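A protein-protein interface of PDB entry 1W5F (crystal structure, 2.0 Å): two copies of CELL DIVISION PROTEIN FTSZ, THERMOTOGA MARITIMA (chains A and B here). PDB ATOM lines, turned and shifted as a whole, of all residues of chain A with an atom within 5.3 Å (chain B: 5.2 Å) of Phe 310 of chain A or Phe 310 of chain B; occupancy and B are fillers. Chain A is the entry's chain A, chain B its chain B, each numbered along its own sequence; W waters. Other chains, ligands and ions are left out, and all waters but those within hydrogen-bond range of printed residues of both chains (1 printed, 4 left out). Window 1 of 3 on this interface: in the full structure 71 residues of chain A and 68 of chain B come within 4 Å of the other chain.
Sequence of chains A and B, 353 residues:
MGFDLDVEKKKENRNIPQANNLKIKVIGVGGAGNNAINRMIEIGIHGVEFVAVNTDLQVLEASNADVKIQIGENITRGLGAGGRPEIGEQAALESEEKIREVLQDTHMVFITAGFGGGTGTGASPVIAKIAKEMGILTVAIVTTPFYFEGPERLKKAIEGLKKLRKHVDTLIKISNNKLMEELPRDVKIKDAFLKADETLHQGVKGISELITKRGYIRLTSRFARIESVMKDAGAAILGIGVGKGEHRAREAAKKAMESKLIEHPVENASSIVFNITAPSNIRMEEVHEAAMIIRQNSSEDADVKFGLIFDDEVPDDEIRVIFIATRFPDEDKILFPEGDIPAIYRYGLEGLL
The side-chain carboxylate (OD2) of Asp 311 of chain B is in hydrogen-bond range of the backbone NH (N) of Tyr 216 of chain A (3.1 Å).
O of Tyr 216 of chain A is in hydrogen-bond range of N of Asp 312 of chain B (2.7 Å).
The side-chain carboxylate (OD2) of Asp 311 of chain A lies within hydrogen-bond range of the backbone NH (N) of Tyr 216 of chain B, 3.0 Å away.
The backbone NH of Asp 312 of chain A sits at hydrogen-bond distance from the backbone carbonyl oxygen of Tyr 216 of chain B.
NH2 of Arg 214 of chain A sits close to NH2 of Arg 214 of chain B, at 2.8 Å.
The backbone NH (N) of Ala 278 of chain A lies within hydrogen-bond range of the backbone carbonyl oxygen (O) of Ile 309 of chain A (3.0 Å).
O of Ala 278 of chain A sits at hydrogen-bond distance from N of Asp 311 of chain A, at 2.8 Å.
OD1 of Asp 312 of chain A is in hydrogen-bond range of N of Ser 280 of chain A (2.7 Å).
The backbone carbonyl oxygen of Ile 309 of chain B is in hydrogen-bond range of the backbone NH of Ala 278 of chain B (3.0 Å).
The backbone NH (N) of Asp 311 of chain B is in hydrogen-bond range of the backbone carbonyl oxygen (O) of Ala 278 of chain B, at 2.8 Å.
The side-chain carboxylate of Asp 312 of chain B is in hydrogen-bond range of the backbone NH of Ser 280 of chain B, at 2.7 Å.
Among the printed residues, merely in contact across the chains: Phe 310 of chain A with Leu 308 of chain B, Arg 214 of chain A with Ile 217 of chain B, Leu 308 of chain A with Phe 310 of chain B, Ile 217 of chain A with Asp 312 of chain B, Ile 217 of chain A with Arg 214 of chain B, Phe 310 of chain A with Phe 310 of chain B, Phe 310 of chain A with Gly 215 of chain B, Gly 215 of chain A with Phe 310 of chain B, Tyr 216 of chain A with Phe 310 of chain B, Asp 312 of chain A with Ile 217 of chain B, Phe 310 of chain A with Ile 217 of chain B, Ile 309 of chain A with Arg 214 of chain B, Asp 311 of chain A with Gly 215 of chain B, Arg 214 of chain A with Ile 309 of chain B, Phe 310 of chain A with Tyr 216 of chain B and Gly 215 of chain A with Asp 311 of chain B.
Printed residues of chain B within 4 Å of Ile 217 of chain A: Arg 214 (3.5 Å) and Asp 312 (3.4 Å).
Of the printed residues of chain B, Ile 309 of chain A touches Arg 214.
Phe 310 of chain A touches five residues of chain B.
Of the printed residues of chain A, Arg 214 of chain B touches Arg 214, Ile 217 and Ile 309.
Of the printed residues of chain A, Ile 217 of chain B touches Arg 214 (3.3 Å), Phe 310 (3.6 Å) and Asp 312 (3.6 Å).
Phe 310 of chain B touches four residues of chain A.
The nearest residue of chain B that does not touch Phe 310 of chain A is Arg 214 of chain B (4.2 Å).
The nearest residue of chain A that does not touch Phe 310 of chain B is Ile 217 of chain A (4.2 Å).
The nearest printed residue of chain A that does not touch Tyr 216 of chain B is Ser 280 of chain A (5.1 Å).
Of the 13 printed residues of chain B, 9 touch a printed residue of chain A.
Hydrophobic or aromatic side chains of chain B that line the printed part of chain A: Tyr 216, Ile 217, Leu 308, Ile 309 and Phe 310.
Along chain B the printed residues that touch a printed residue of chain A span positions 214 to 312.
Hydrophobic or aromatic side chains of chain A within 4 Å of the printed part of chain B: Tyr 216, Ile 217, Leu 308, Ile 309 and Phe 310.
Among the printed residues, no Asp or Glu carboxylate lies within 4 Å of a Lys or Arg side-chain nitrogen of the other chain.
Arg 214 of chain B touches its own counterpart, Arg 214 of chain A.
Tyr 216 of chain A touches Asp 311 of chain B, and with the chains exchanged Asp 311 of chain A touches Tyr 216 of chain B.
Ile 217 of chain A touches Asp 312 of chain B, and with the chains exchanged Asp 312 of chain A touches Ile 217 of chain B.
Leu 308 of chain A touches Phe 310 of chain B, and with the chains exchanged Phe 310 of chain A touches Leu 308 of chain B.
Positions printed for both chains: 214, 215, 216, 217, 278, 279, 280, 282, 308, 309, 310, 311 and 312.
Water W1 lies within hydrogen-bond range of O of Ile 217 of chain A (2.9 Å) and NE of Arg 214 of chain B (3.4 Å).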
ATOM      1  N   ARG A 214     -10.737  23.631 -13.018  1.00  0.00           N
ATOM      2  CA  ARG A 214     -12.167  23.613 -12.749  1.00  0.00           C
ATOM      3  C   ARG A 214     -12.959  23.450 -14.036  1.00  0.00           C
ATOM      4  O   ARG A 214     -13.955  22.735 -14.078  1.00  0.00           O
ATOM      5  CB  ARG A 214     -12.563  24.928 -12.075  1.00  0.00           C
ATOM      6  CG  ARG A 214     -14.056  25.206 -12.042  1.00  0.00           C
ATOM      7  CD  ARG A 214     -14.361  26.618 -12.527  1.00  0.00           C
ATOM      8  NE  ARG A 214     -13.604  27.624 -11.789  1.00  0.00           N
ATOM      9  CZ  ARG A 214     -13.636  28.927 -12.052  1.00  0.00           C
ATOM     10  NH1 ARG A 214     -12.913  29.769 -11.325  1.00  0.00           N
ATOM     11  NH2 ARG A 214     -14.386  29.388 -13.044  1.00  0.00           N
ATOM     12  N   GLY A 215     -12.498  24.118 -15.089  1.00  0.00           N
ATOM     13  CA  GLY A 215     -13.197  24.080 -16.355  1.00  0.00           C
ATOM     14  C   GLY A 215     -13.953  25.392 -16.473  1.00  0.00           C
ATOM     15  O   GLY A 215     -14.564  25.858 -15.504  1.00  0.00           O
ATOM     16  N   TYR A 216     -13.899  25.999 -17.653  1.00  0.00           N
ATOM     17  CA  TYR A 216     -14.569  27.267 -17.903  1.00  0.00           C
ATOM     18  C   TYR A 216     -16.016  27.067 -18.350  1.00  0.00           C
ATOM     19  O   TYR A 216     -16.314  26.167 -19.129  1.00  0.00           O
ATOM     20  CB  TYR A 216     -13.793  28.045 -18.975  1.00  0.00           C
ATOM     21  CG  TYR A 216     -14.519  29.259 -19.512  1.00  0.00           C
ATOM     22  CD1 TYR A 216     -14.849  30.326 -18.676  1.00  0.00           C
ATOM     23  CD2 TYR A 216     -14.893  29.333 -20.855  1.00  0.00           C
ATOM     24  CE1 TYR A 216     -15.538  31.438 -19.163  1.00  0.00           C
ATOM     25  CE2 TYR A 216     -15.582  30.440 -21.353  1.00  0.00           C
ATOM     26  CZ  TYR A 216     -15.902  31.486 -20.500  1.00  0.00           C
ATOM     27  OH  TYR A 216     -16.598  32.572 -20.979  1.00  0.00           O
ATOM     28  N   ILE A 217     -16.919  27.900 -17.845  1.00  0.00           N
ATOM     29  CA  ILE A 217     -18.320  27.798 -18.234  1.00  0.00           C
ATOM     30  C   ILE A 217     -18.822  29.061 -18.926  1.00  0.00           C
ATOM     31  O   ILE A 217     -18.932  30.118 -18.308  1.00  0.00           O
ATOM     32  CB  ILE A 217     -19.218  27.496 -17.019  1.00  0.00           C
ATOM     33  CG1 ILE A 217     -18.894  26.092 -16.491  1.00  0.00           C
ATOM     34  CG2 ILE A 217     -20.685  27.592 -17.416  1.00  0.00           C
ATOM     35  CD1 ILE A 217     -19.744  25.651 -15.325  1.00  0.00           C
ATOM     36  N   ALA A 278     -26.031  19.938  -8.401  1.00  0.00           N
ATOM     37  CA  ALA A 278     -25.552  19.156  -7.271  1.00  0.00           C
ATOM     38  C   ALA A 278     -24.070  19.315  -6.975  1.00  0.00           C
ATOM     39  O   ALA A 278     -23.308  19.824  -7.799  1.00  0.00           O
ATOM     40  CB  ALA A 278     -25.857  17.688  -7.526  1.00  0.00           C
ATOM     41  N   PRO A 279     -23.644  18.883  -5.776  1.00  0.00           N
ATOM     42  CA  PRO A 279     -22.229  18.986  -5.415  1.00  0.00           C
ATOM     43  C   PRO A 279     -21.428  18.055  -6.319  1.00  0.00           C
ATOM     44  O   PRO A 279     -21.994  17.179  -6.968  1.00  0.00           O
ATOM     45  CB  PRO A 279     -22.208  18.568  -3.941  1.00  0.00           C
ATOM     46  CG  PRO A 279     -23.418  17.695  -3.798  1.00  0.00           C
ATOM     47  CD  PRO A 279     -24.448  18.403  -4.637  1.00  0.00           C
ATOM     48  N   SER A 280     -20.118  18.253  -6.372  1.00  0.00           N
ATOM     49  CA  SER A 280     -19.256  17.442  -7.225  1.00  0.00           C
ATOM     50  C   SER A 280     -19.197  15.960  -6.855  1.00  0.00           C
ATOM     51  O   SER A 280     -18.688  15.148  -7.629  1.00  0.00           O
ATOM     52  CB  SER A 280     -17.834  18.015  -7.222  1.00  0.00           C
ATOM     53  OG  SER A 280     -17.802  19.316  -7.781  1.00  0.00           O
ATOM     54  N   ILE A 282     -21.660  13.965  -6.660  1.00  0.00           N
ATOM     55  CA  ILE A 282     -22.781  13.228  -7.228  1.00  0.00           C
ATOM     56  C   ILE A 282     -22.286  12.054  -8.078  1.00  0.00           C
ATOM     57  O   ILE A 282     -21.340  12.188  -8.855  1.00  0.00           O
ATOM     58  CB  ILE A 282     -23.691  14.160  -8.075  1.00  0.00           C
ATOM     59  CG1 ILE A 282     -24.948  13.404  -8.512  1.00  0.00           C
ATOM     60  CG2 ILE A 282     -22.917  14.709  -9.265  1.00  0.00           C
ATOM     61  CD1 ILE A 282     -25.942  14.242  -9.289  1.00  0.00           C
ATOM     62  N   LEU A 308     -26.874  19.522 -16.301  1.00  0.00           N
ATOM     63  CA  LEU A 308     -26.162  19.161 -15.087  1.00  0.00           C
ATOM     64  C   LEU A 308     -25.231  20.304 -14.727  1.00  0.00           C
ATOM     65  O   LEU A 308     -24.430  20.746 -15.548  1.00  0.00           O
ATOM     66  CB  LEU A 308     -25.364  17.869 -15.301  1.00  0.00           C
ATOM     67  CG  LEU A 308     -24.686  17.204 -14.097  1.00  0.00           C
ATOM     68  CD1 LEU A 308     -23.619  18.118 -13.534  1.00  0.00           C
ATOM     69  CD2 LEU A 308     -25.725  16.876 -13.030  1.00  0.00           C
ATOM     70  N   ILE A 309     -25.352  20.783 -13.498  1.00  0.00           N
ATOM     71  CA  ILE A 309     -24.522  21.871 -13.005  1.00  0.00           C
ATOM     72  C   ILE A 309     -23.903  21.450 -11.683  1.00  0.00           C
ATOM     73  O   ILE A 309     -24.624  21.120 -10.739  1.00  0.00           O
ATOM     74  CB  ILE A 309     -25.353  23.149 -12.746  1.00  0.00           C
ATOM     75  CG1 ILE A 309     -25.958  23.660 -14.058  1.00  0.00           C
ATOM     76  CG2 ILE A 309     -24.468  24.219 -12.105  1.00  0.00           C
ATOM     77  CD1 ILE A 309     -26.930  24.815 -13.880  1.00  0.00           C
ATOM     78  N   PHE A 310     -22.575  21.448 -11.620  1.00  0.00           N
ATOM     79  CA  PHE A 310     -21.880  21.095 -10.385  1.00  0.00           C
ATOM     80  C   PHE A 310     -21.712  22.380  -9.585  1.00  0.00           C
ATOM     81  O   PHE A 310     -21.104  23.345 -10.060  1.00  0.00           O
ATOM     82  CB  PHE A 310     -20.496  20.509 -10.671  1.00  0.00           C
ATOM     83  CG  PHE A 310     -20.524  19.207 -11.412  1.00  0.00           C
ATOM     84  CD1 PHE A 310     -20.389  19.176 -12.796  1.00  0.00           C
ATOM     85  CD2 PHE A 310     -20.670  18.008 -10.725  1.00  0.00           C
ATOM     86  CE1 PHE A 310     -20.396  17.969 -13.485  1.00  0.00           C
ATOM     87  CE2 PHE A 310     -20.677  16.793 -11.406  1.00  0.00           C
ATOM     88  CZ  PHE A 310     -20.540  16.775 -12.790  1.00  0.00           C
ATOM     89  N   ASP A 311     -22.250  22.392  -8.373  1.00  0.00           N
ATOM     90  CA  ASP A 311     -22.160  23.562  -7.518  1.00  0.00           C
ATOM     91  C   ASP A 311     -21.926  23.098  -6.095  1.00  0.00           C
ATOM     92  O   ASP A 311     -22.855  22.669  -5.414  1.00  0.00           O
ATOM     93  CB  ASP A 311     -23.454  24.376  -7.593  1.00  0.00           C
ATOM     94  CG  ASP A 311     -23.378  25.665  -6.795  1.00  0.00           C
ATOM     95  OD1 ASP A 311     -24.419  26.333  -6.642  1.00  0.00           O
ATOM     96  OD2 ASP A 311     -22.274  26.013  -6.323  1.00  0.00           O
ATOM     97  N   ASP A 312     -20.680  23.183  -5.648  1.00  0.00           N
ATOM     98  CA  ASP A 312     -20.348  22.746  -4.306  1.00  0.00           C
ATOM     99  C   ASP A 312     -20.791  23.691  -3.203  1.00  0.00           C
ATOM    100  O   ASP A 312     -20.397  23.533  -2.049  1.00  0.00           O
ATOM    101  CB  ASP A 312     -18.857  22.432  -4.217  1.00  0.00           C
ATOM    102  CG  ASP A 312     -18.508  21.168  -4.964  1.00  0.00           C
ATOM    103  OD1 ASP A 312     -19.163  20.142  -4.694  1.00  0.00           O
ATOM    104  OD2 ASP A 312     -17.604  21.194  -5.825  1.00  0.00           O
ATOM    105  N   ARG B 214     -22.806  29.990 -12.426  1.00  0.00           N
ATOM    106  CA  ARG B 214     -21.948  28.972 -13.023  1.00  0.00           C
ATOM    107  C   ARG B 214     -21.819  27.741 -12.134  1.00  0.00           C
ATOM    108  O   ARG B 214     -21.734  26.613 -12.622  1.00  0.00           O
ATOM    109  CB  ARG B 214     -20.563  29.574 -13.277  1.00  0.00           C
ATOM    110  CG  ARG B 214     -19.441  28.571 -13.454  1.00  0.00           C
ATOM    111  CD  ARG B 214     -18.273  28.914 -12.536  1.00  0.00           C
ATOM    112  NE  ARG B 214     -17.843  30.301 -12.698  1.00  0.00           N
ATOM    113  CZ  ARG B 214     -16.854  30.869 -12.012  1.00  0.00           C
ATOM    114  NH1 ARG B 214     -16.538  32.140 -12.231  1.00  0.00           N
ATOM    115  NH2 ARG B 214     -16.178  30.171 -11.108  1.00  0.00           N
ATOM    116  N   GLY B 215     -21.823  27.970 -10.826  1.00  0.00           N
ATOM    117  CA  GLY B 215     -21.666  26.883  -9.879  1.00  0.00           C
ATOM    118  C   GLY B 215     -20.215  26.856  -9.427  1.00  0.00           C
ATOM    119  O   GLY B 215     -19.297  27.011 -10.242  1.00  0.00           O
ATOM    120  N   TYR B 216     -20.006  26.682  -8.127  1.00  0.00           N
ATOM    121  CA  TYR B 216     -18.668  26.633  -7.550  1.00  0.00           C
ATOM    122  C   TYR B 216     -18.093  25.213  -7.572  1.00  0.00           C
ATOM    123  O   TYR B 216     -18.790  24.248  -7.267  1.00  0.00           O
ATOM    124  CB  TYR B 216     -18.721  27.144  -6.105  1.00  0.00           C
ATOM    125  CG  TYR B 216     -17.477  26.858  -5.292  1.00  0.00           C
ATOM    126  CD1 TYR B 216     -16.263  27.484  -5.583  1.00  0.00           C
ATOM    127  CD2 TYR B 216     -17.519  25.965  -4.220  1.00  0.00           C
ATOM    128  CE1 TYR B 216     -15.118  27.227  -4.819  1.00  0.00           C
ATOM    129  CE2 TYR B 216     -16.383  25.702  -3.450  1.00  0.00           C
ATOM    130  CZ  TYR B 216     -15.191  26.335  -3.753  1.00  0.00           C
ATOM    131  OH  TYR B 216     -14.082  26.084  -2.978  1.00  0.00           O
ATOM    132  N   ILE B 217     -16.824  25.084  -7.940  1.00  0.00           N
ATOM    133  CA  ILE B 217     -16.183  23.773  -7.975  1.00  0.00           C
ATOM    134  C   ILE B 217     -15.148  23.686  -6.860  1.00  0.00           C
ATOM    135  O   ILE B 217     -14.184  24.447  -6.849  1.00  0.00           O
ATOM    136  CB  ILE B 217     -15.439  23.516  -9.300  1.00  0.00           C
ATOM    137  CG1 ILE B 217     -16.406  23.561 -10.491  1.00  0.00           C
ATOM    138  CG2 ILE B 217     -14.727  22.169  -9.223  1.00  0.00           C
ATOM    139  CD1 ILE B 217     -17.368  22.387 -10.586  1.00  0.00           C
ATOM    140  N   ALA B 278     -15.845  18.172 -21.551  1.00  0.00           N
ATOM    141  CA  ALA B 278     -16.466  18.656 -22.777  1.00  0.00           C
ATOM    142  C   ALA B 278     -17.151  20.005 -22.620  1.00  0.00           C
ATOM    143  O   ALA B 278     -17.393  20.470 -21.503  1.00  0.00           O
ATOM    144  CB  ALA B 278     -17.478  17.628 -23.256  1.00  0.00           C
ATOM    145  N   PRO B 279     -17.471  20.654 -23.749  1.00  0.00           N
ATOM    146  CA  PRO B 279     -18.143  21.952 -23.692  1.00  0.00           C
ATOM    147  C   PRO B 279     -19.544  21.773 -23.121  1.00  0.00           C
ATOM    148  O   PRO B 279     -20.081  20.663 -23.103  1.00  0.00           O
ATOM    149  CB  PRO B 279     -18.148  22.410 -25.152  1.00  0.00           C
ATOM    150  CG  PRO B 279     -18.120  21.131 -25.919  1.00  0.00           C
ATOM    151  CD  PRO B 279     -17.146  20.292 -25.141  1.00  0.00           C
ATOM    152  N   SER B 280     -20.131  22.869 -22.661  1.00  0.00           N
ATOM    153  CA  SER B 280     -21.455  22.844 -22.056  1.00  0.00           C
ATOM    154  C   SER B 280     -22.565  22.325 -22.961  1.00  0.00           C
ATOM    155  O   SER B 280     -23.635  21.959 -22.475  1.00  0.00           O
ATOM    156  CB  SER B 280     -21.819  24.243 -21.553  1.00  0.00           C
ATOM    157  OG  SER B 280     -20.926  24.653 -20.525  1.00  0.00           O
ATOM    158  N   ILE B 282     -22.692  19.557 -24.483  1.00  0.00           N
ATOM    159  CA  ILE B 282     -22.768  18.097 -24.523  1.00  0.00           C
ATOM    160  C   ILE B 282     -24.143  17.590 -24.089  1.00  0.00           C
ATOM    161  O   ILE B 282     -24.722  18.069 -23.108  1.00  0.00           O
ATOM    162  CB  ILE B 282     -21.670  17.435 -23.647  1.00  0.00           C
ATOM    163  CG1 ILE B 282     -21.688  15.918 -23.865  1.00  0.00           C
ATOM    164  CG2 ILE B 282     -21.876  17.791 -22.181  1.00  0.00           C
ATOM    165  CD1 ILE B 282     -20.563  15.171 -23.177  1.00  0.00           C
ATOM    166  N   LEU B 308     -17.420  13.871 -14.878  1.00  0.00           N
ATOM    167  CA  LEU B 308     -17.860  14.816 -15.895  1.00  0.00           C
ATOM    168  C   LEU B 308     -17.393  16.226 -15.546  1.00  0.00           C
ATOM    169  O   LEU B 308     -17.613  16.706 -14.431  1.00  0.00           O
ATOM    170  CB  LEU B 308     -19.385  14.791 -16.011  1.00  0.00           C
ATOM    171  CG  LEU B 308     -19.993  14.946 -17.406  1.00  0.00           C
ATOM    172  CD1 LEU B 308     -19.451  16.197 -18.082  1.00  0.00           C
ATOM    173  CD2 LEU B 308     -19.671  13.706 -18.237  1.00  0.00           C
ATOM    174  N   ILE B 309     -16.748  16.876 -16.511  1.00  0.00           N
ATOM    175  CA  ILE B 309     -16.245  18.233 -16.339  1.00  0.00           C
ATOM    176  C   ILE B 309     -16.658  19.070 -17.544  1.00  0.00           C
ATOM    177  O   ILE B 309     -16.379  18.702 -18.688  1.00  0.00           O
ATOM    178  CB  ILE B 309     -14.697  18.257 -16.244  1.00  0.00           C
ATOM    179  CG1 ILE B 309     -14.233  17.524 -14.980  1.00  0.00           C
ATOM    180  CG2 ILE B 309     -14.193  19.701 -16.234  1.00  0.00           C
ATOM    181  CD1 ILE B 309     -12.716  17.438 -14.851  1.00  0.00           C
ATOM    182  N   PHE B 310     -17.338  20.184 -17.291  1.00  0.00           N
ATOM    183  CA  PHE B 310     -17.752  21.061 -18.376  1.00  0.00           C
ATOM    184  C   PHE B 310     -16.685  22.130 -18.534  1.00  0.00           C
ATOM    185  O   PHE B 310     -16.382  22.864 -17.591  1.00  0.00           O
ATOM    186  CB  PHE B 310     -19.111  21.697 -18.077  1.00  0.00           C
ATOM    187  CG  PHE B 310     -20.214  20.694 -17.914  1.00  0.00           C
ATOM    188  CD1 PHE B 310     -20.600  20.260 -16.650  1.00  0.00           C
ATOM    189  CD2 PHE B 310     -20.836  20.146 -19.030  1.00  0.00           C
ATOM    190  CE1 PHE B 310     -21.586  19.291 -16.500  1.00  0.00           C
ATOM    191  CE2 PHE B 310     -21.826  19.173 -18.890  1.00  0.00           C
ATOM    192  CZ  PHE B 310     -22.200  18.746 -17.623  1.00  0.00           C
ATOM    193  N   ASP B 311     -16.106  22.201 -19.726  1.00  0.00           N
ATOM    194  CA  ASP B 311     -15.052  23.162 -20.009  1.00  0.00           C
ATOM    195  C   ASP B 311     -15.245  23.727 -21.404  1.00  0.00           C
ATOM    196  O   ASP B 311     -14.900  23.084 -22.394  1.00  0.00           O
ATOM    197  CB  ASP B 311     -13.693  22.477 -19.921  1.00  0.00           C
ATOM    198  CG  ASP B 311     -12.542  23.441 -20.101  1.00  0.00           C
ATOM    199  OD1 ASP B 311     -11.391  22.971 -20.171  1.00  0.00           O
ATOM    200  OD2 ASP B 311     -12.789  24.666 -20.167  1.00  0.00           O
ATOM    201  N   ASP B 312     -15.790  24.934 -21.488  1.00  0.00           N
ATOM    202  CA  ASP B 312     -16.019  25.533 -22.790  1.00  0.00           C
ATOM    203  C   ASP B 312     -14.753  26.009 -23.481  1.00  0.00           C
ATOM    204  O   ASP B 312     -14.811  26.668 -24.516  1.00  0.00           O
ATOM    205  CB  ASP B 312     -17.053  26.643 -22.669  1.00  0.00           C
ATOM    206  CG  ASP B 312     -18.427  26.093 -22.366  1.00  0.00           C
ATOM    207  OD1 ASP B 312     -18.895  25.252 -23.160  1.00  0.00           O
ATOM    208  OD2 ASP B 312     -19.030  26.482 -21.341  1.00  0.00           O
HETATM  209  O   HOH W   1     -18.643  31.489 -15.753  1.00  0.00           O
